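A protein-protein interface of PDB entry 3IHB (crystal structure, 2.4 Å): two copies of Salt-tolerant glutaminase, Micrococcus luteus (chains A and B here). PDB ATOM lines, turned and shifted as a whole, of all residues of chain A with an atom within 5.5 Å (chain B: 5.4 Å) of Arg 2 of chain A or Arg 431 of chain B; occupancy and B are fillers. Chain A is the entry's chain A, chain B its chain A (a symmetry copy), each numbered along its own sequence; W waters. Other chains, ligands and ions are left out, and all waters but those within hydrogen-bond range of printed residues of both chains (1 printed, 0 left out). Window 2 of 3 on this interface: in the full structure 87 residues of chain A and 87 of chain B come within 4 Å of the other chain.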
ATOM      1  N   MET A   1      11.663  10.806  13.111  1.00  0.00           N
ATOM      2  CA  MET A   1      12.413  12.025  12.701  1.00  0.00           C
ATOM      3  C   MET A   1      11.603  12.790  11.672  1.00  0.00           C
ATOM      4  O   MET A   1      10.843  12.197  10.903  1.00  0.00           O
ATOM      5  CB  MET A   1      13.749  11.643  12.078  1.00  0.00           C
ATOM      6  CG  MET A   1      13.606  10.939  10.741  1.00  0.00           C
ATOM      7  SD  MET A   1      15.188  10.525  10.034  1.00  0.00           S
ATOM      8  CE  MET A   1      15.605  12.047   9.192  1.00  0.00           C
ATOM      9  N   ARG A   2      11.770  14.108  11.656  1.00  0.00           N
ATOM     10  CA  ARG A   2      11.060  14.945  10.701  1.00  0.00           C
ATOM     11  C   ARG A   2      11.971  15.221   9.516  1.00  0.00           C
ATOM     12  O   ARG A   2      13.185  15.364   9.676  1.00  0.00           O
ATOM     13  CB  ARG A   2      10.639  16.263  11.350  1.00  0.00           C
ATOM     14  CG  ARG A   2      11.782  17.213  11.625  1.00  0.00           C
ATOM     15  CD  ARG A   2      11.267  18.458  12.314  1.00  0.00           C
ATOM     16  NE  ARG A   2      10.074  18.967  11.650  1.00  0.00           N
ATOM     17  CZ  ARG A   2       9.338  19.973  12.105  1.00  0.00           C
ATOM     18  NH1 ARG A   2       9.677  20.581  13.234  1.00  0.00           N
ATOM     19  NH2 ARG A   2       8.260  20.365  11.440  1.00  0.00           N
ATOM     20  N   HIS A   3      11.376  15.277   8.328  1.00  0.00           N
ATOM     21  CA  HIS A   3      12.125  15.539   7.106  1.00  0.00           C
ATOM     22  C   HIS A   3      12.755  16.918   7.239  1.00  0.00           C
ATOM     23  O   HIS A   3      12.079  17.898   7.561  1.00  0.00           O
ATOM     24  CB  HIS A   3      11.188  15.508   5.890  1.00  0.00           C
ATOM     25  CG  HIS A   3      11.889  15.223   4.599  1.00  0.00           C
ATOM     26  ND1 HIS A   3      12.857  16.056   4.077  1.00  0.00           N
ATOM     27  CD2 HIS A   3      11.807  14.166   3.753  1.00  0.00           C
ATOM     28  CE1 HIS A   3      13.345  15.521   2.969  1.00  0.00           C
ATOM     29  NE2 HIS A   3      12.725  14.374   2.752  1.00  0.00           N
ATOM     30  N   PRO A   4      14.069  17.008   7.017  1.00  0.00           N
ATOM     31  CA  PRO A   4      14.778  18.286   7.114  1.00  0.00           C
ATOM     32  C   PRO A   4      14.532  19.341   6.018  1.00  0.00           C
ATOM     33  O   PRO A   4      14.793  20.527   6.252  1.00  0.00           O
ATOM     34  CB  PRO A   4      16.249  17.863   7.194  1.00  0.00           C
ATOM     35  CG  PRO A   4      16.282  16.530   6.504  1.00  0.00           C
ATOM     36  CD  PRO A   4      15.011  15.873   6.964  1.00  0.00           C
ATOM     37  N   ASP A   7      12.069  22.087   6.989  1.00  0.00           N
ATOM     38  CA  ASP A   7      12.641  22.939   8.026  1.00  0.00           C
ATOM     39  C   ASP A   7      13.534  23.975   7.350  1.00  0.00           C
ATOM     40  O   ASP A   7      13.648  25.113   7.807  1.00  0.00           O
ATOM     41  CB  ASP A   7      13.460  22.121   9.029  1.00  0.00           C
ATOM     42  CG  ASP A   7      12.588  21.334   9.980  1.00  0.00           C
ATOM     43  OD1 ASP A   7      11.363  21.572   9.986  1.00  0.00           O
ATOM     44  OD2 ASP A   7      13.124  20.491  10.725  1.00  0.00           O
ATOM     45  N   THR B 348      13.136   9.018   6.658  1.00  0.00           N
ATOM     46  CA  THR B 348      11.892   9.501   7.246  1.00  0.00           C
ATOM     47  C   THR B 348      10.778   8.459   7.131  1.00  0.00           C
ATOM     48  O   THR B 348       9.993   8.295   8.058  1.00  0.00           O
ATOM     49  CB  THR B 348      11.411  10.817   6.566  1.00  0.00           C
ATOM     50  OG1 THR B 348      12.444  11.807   6.644  1.00  0.00           O
ATOM     51  CG2 THR B 348      10.167  11.361   7.262  1.00  0.00           C
ATOM     52  N   ALA B 426      24.065  13.985   6.475  1.00  0.00           N
ATOM     53  CA  ALA B 426      24.587  14.116   7.832  1.00  0.00           C
ATOM     54  C   ALA B 426      23.444  14.465   8.768  1.00  0.00           C
ATOM     55  O   ALA B 426      23.221  13.788   9.769  1.00  0.00           O
ATOM     56  CB  ALA B 426      25.660  15.201   7.891  1.00  0.00           C
ATOM     57  N   GLU B 427      22.717  15.523   8.429  1.00  0.00           N
ATOM     58  CA  GLU B 427      21.590  15.982   9.230  1.00  0.00           C
ATOM     59  C   GLU B 427      20.550  14.889   9.422  1.00  0.00           C
ATOM     60  O   GLU B 427      19.966  14.770  10.491  1.00  0.00           O
ATOM     61  CB  GLU B 427      20.935  17.197   8.567  1.00  0.00           C
ATOM     62  CG  GLU B 427      19.687  17.719   9.275  1.00  0.00           C
ATOM     63  CD  GLU B 427      19.975  18.224  10.681  1.00  0.00           C
ATOM     64  OE1 GLU B 427      21.098  18.722  10.924  1.00  0.00           O
ATOM     65  OE2 GLU B 427      19.075  18.137  11.541  1.00  0.00           O
ATOM     66  N   GLY B 428      20.316  14.095   8.383  1.00  0.00           N
ATOM     67  CA  GLY B 428      19.331  13.032   8.485  1.00  0.00           C
ATOM     68  C   GLY B 428      19.731  11.994   9.519  1.00  0.00           C
ATOM     69  O   GLY B 428      18.876  11.389  10.180  1.00  0.00           O
ATOM     70  N   VAL B 429      21.038  11.785   9.649  1.00  0.00           N
ATOM     71  CA  VAL B 429      21.578  10.823  10.596  1.00  0.00           C
ATOM     72  C   VAL B 429      21.541  11.404  12.001  1.00  0.00           C
ATOM     73  O   VAL B 429      21.299  10.685  12.969  1.00  0.00           O
ATOM     74  CB  VAL B 429      23.025  10.440  10.231  1.00  0.00           C
ATOM     75  CG1 VAL B 429      23.607   9.524  11.294  1.00  0.00           C
ATOM     76  CG2 VAL B 429      23.048   9.752   8.877  1.00  0.00           C
ATOM     77  N   ARG B 430      21.785  12.707  12.106  1.00  0.00           N
ATOM     78  CA  ARG B 430      21.744  13.391  13.395  1.00  0.00           C
ATOM     79  C   ARG B 430      20.329  13.247  13.971  1.00  0.00           C
ATOM     80  O   ARG B 430      20.151  13.015  15.167  1.00  0.00           O
ATOM     81  CB  ARG B 430      22.080  14.873  13.211  1.00  0.00           C
ATOM     82  CG  ARG B 430      21.916  15.712  14.459  1.00  0.00           C
ATOM     83  CD  ARG B 430      21.544  17.153  14.119  1.00  0.00           C
ATOM     84  NE  ARG B 430      21.038  17.861  15.292  1.00  0.00           N
ATOM     85  CZ  ARG B 430      20.264  18.940  15.243  1.00  0.00           C
ATOM     86  NH1 ARG B 430      19.895  19.451  14.074  1.00  0.00           N
ATOM     87  NH2 ARG B 430      19.845  19.503  16.369  1.00  0.00           N
ATOM     88  N   ARG B 431      19.327  13.372  13.104  1.00  0.00           N
ATOM     89  CA  ARG B 431      17.934  13.262  13.513  1.00  0.00           C
ATOM     90  C   ARG B 431      17.496  11.824  13.803  1.00  0.00           C
ATOM     91  O   ARG B 431      16.505  11.605  14.496  1.00  0.00           O
ATOM     92  CB  ARG B 431      17.025  13.885  12.445  1.00  0.00           C
ATOM     93  CG  ARG B 431      17.311  15.362  12.188  1.00  0.00           C
ATOM     94  CD  ARG B 431      16.292  16.008  11.255  1.00  0.00           C
ATOM     95  NE  ARG B 431      16.545  17.441  11.125  1.00  0.00           N
ATOM     96  CZ  ARG B 431      15.624  18.341  10.801  1.00  0.00           C
ATOM     97  NH1 ARG B 431      14.372  17.964  10.564  1.00  0.00           N
ATOM     98  NH2 ARG B 431      15.946  19.622  10.742  1.00  0.00           N
ATOM     99  N   LEU B 432      18.215  10.843  13.267  1.00  0.00           N
ATOM    100  CA  LEU B 432      17.873   9.441  13.515  1.00  0.00           C
ATOM    101  C   LEU B 432      18.242   9.112  14.954  1.00  0.00           C
ATOM    102  O   LEU B 432      17.428   8.598  15.731  1.00  0.00           O
ATOM    103  CB  LEU B 432      18.666   8.518  12.593  1.00  0.00           C
ATOM    104  CG  LEU B 432      18.229   8.359  11.146  1.00  0.00           C
ATOM    105  CD1 LEU B 432      19.357   7.724  10.351  1.00  0.00           C
ATOM    106  CD2 LEU B 432      16.966   7.507  11.088  1.00  0.00           C
ATOM    107  N   GLN B 433      19.492   9.417  15.281  1.00  0.00           N
ATOM    108  CA  GLN B 433      20.044   9.186  16.601  1.00  0.00           C
ATOM    109  C   GLN B 433      19.179   9.879  17.644  1.00  0.00           C
ATOM    110  O   GLN B 433      19.045   9.401  18.770  1.00  0.00           O
ATOM    111  CB  GLN B 433      21.474   9.730  16.649  1.00  0.00           C
ATOM    112  CG  GLN B 433      22.371   9.158  15.560  1.00  0.00           C
ATOM    113  CD  GLN B 433      23.785   9.698  15.619  1.00  0.00           C
ATOM    114  OE1 GLN B 433      24.006  10.904  15.513  1.00  0.00           O
ATOM    115  NE2 GLN B 433      24.751   8.808  15.789  1.00  0.00           N
ATOM    116  N   ALA B 434      18.589  11.005  17.254  1.00  0.00           N
ATOM    117  CA  ALA B 434      17.730  11.761  18.152  1.00  0.00           C
ATOM    118  C   ALA B 434      16.479  10.953  18.482  1.00  0.00           C
ATOM    119  O   ALA B 434      15.841  11.181  19.505  1.00  0.00           O
ATOM    120  CB  ALA B 434      17.350  13.097  17.516  1.00  0.00           C
ATOM    121  N   ASP B 435      16.127  10.012  17.613  1.00  0.00           N
ATOM    122  CA  ASP B 435      14.958   9.173  17.850  1.00  0.00           C
ATOM    123  C   ASP B 435      15.338   7.991  18.724  1.00  0.00           C
ATOM    124  O   ASP B 435      14.522   7.104  18.976  1.00  0.00           O
ATOM    125  CB  ASP B 435      14.377   8.659  16.534  1.00  0.00           C
ATOM    126  CG  ASP B 435      13.682   9.745  15.740  1.00  0.00           C
ATOM    127  OD1 ASP B 435      12.766  10.395  16.290  1.00  0.00           O
ATOM    128  OD2 ASP B 435      14.048   9.942  14.563  1.00  0.00           O
HETATM  129  O   HOH W   1      11.861   8.286  10.716  1.00  0.00           O
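No position is printed for both chains.
Of the printed residues of chain B, His 3 of chain A touches Thr 348 (3.8 Å) and Arg 431 (3.8 Å).
Printed residues of chain B within 4 Å of Asp 7 of chain A: Arg 431.
Printed residues of chain A within 4 Å of Thr 348 of chain B: Met 1 and His 3.
Arg 430 of chain B touches none of the printed residues of chain A.
Printed residues of chain A within 4 Å of Leu 432 of chain B: Met 1.
Of the printed residues of chain A, Asp 435 of chain B touches Met 1 (2.9 Å).
The nearest residue of chain B that does not touch Arg 2 of chain A is Thr 348 of chain B (4.5 Å).
The nearest printed residue of chain B that does not touch Asp 7 of chain A is Glu 427 of chain B (6.5 Å).
Among the printed residues, pairs that only touch across the chains: Met 1 of chain A with Thr 348 of chain B, Met 1 of chain A with Arg 431 of chain B, Met 1 of chain A with Leu 432 of chain B, His 3 of chain A with Thr 348 of chain B, His 3 of chain A with Arg 431 of chain B and Pro 4 of chain A with Arg 431 of chain B.
Of the 5 printed residues of chain A, 5 touch a printed residue of chain B.
Hydrophobic or aromatic side chains of chain A within 4 Å of the printed part of chain B: Met 1, His 3 and Pro 4.
Of the 11 printed residues of chain B, 5 touch a printed residue of chain A.
Along chain B the printed residues that touch a printed residue of chain A span positions 348 to 435.
Among the printed residues, 10 pairs touch across the chains.
Among the printed residues, Asp or Glu carboxylates within 4 Å of a Lys or Arg side-chain nitrogen of the other chain: Asp 7 of chain A with Arg 431 of chain B.
The guanidinium group (NE) of Arg 2 of chain A lies within salt-bridge range of the side-chain carboxylate (OD1) of Asp 7 of chain A (3.3 Å).
OE2 of Glu 427 of chain B is in salt-bridge range of NE of Arg 431 of chain B.
Water W1 lies within hydrogen-bond range of the backbone carbonyl oxygen (O) of Thr 348 of chain B and the backbone NH (N) of Met 1 of chain A.
OD2 of Asp 435 of chain B is in hydrogen-bond range of N of Met 1 of chain A, 2.9 Å away.
The backbone carbonyl oxygen (O) of Arg 2 of chain A sits close to the guanidinium group (NH1) of Arg 431 of chain B, at 3.0 Å.
The side-chain carboxylate of Asp 7 of chain A lies within salt-bridge range of the guanidinium group of Arg 431 of chain B, at 2.8 Å.
SD of Met 1 of chain A sits close to O of Gly 428 of chain B (3.8 Å).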
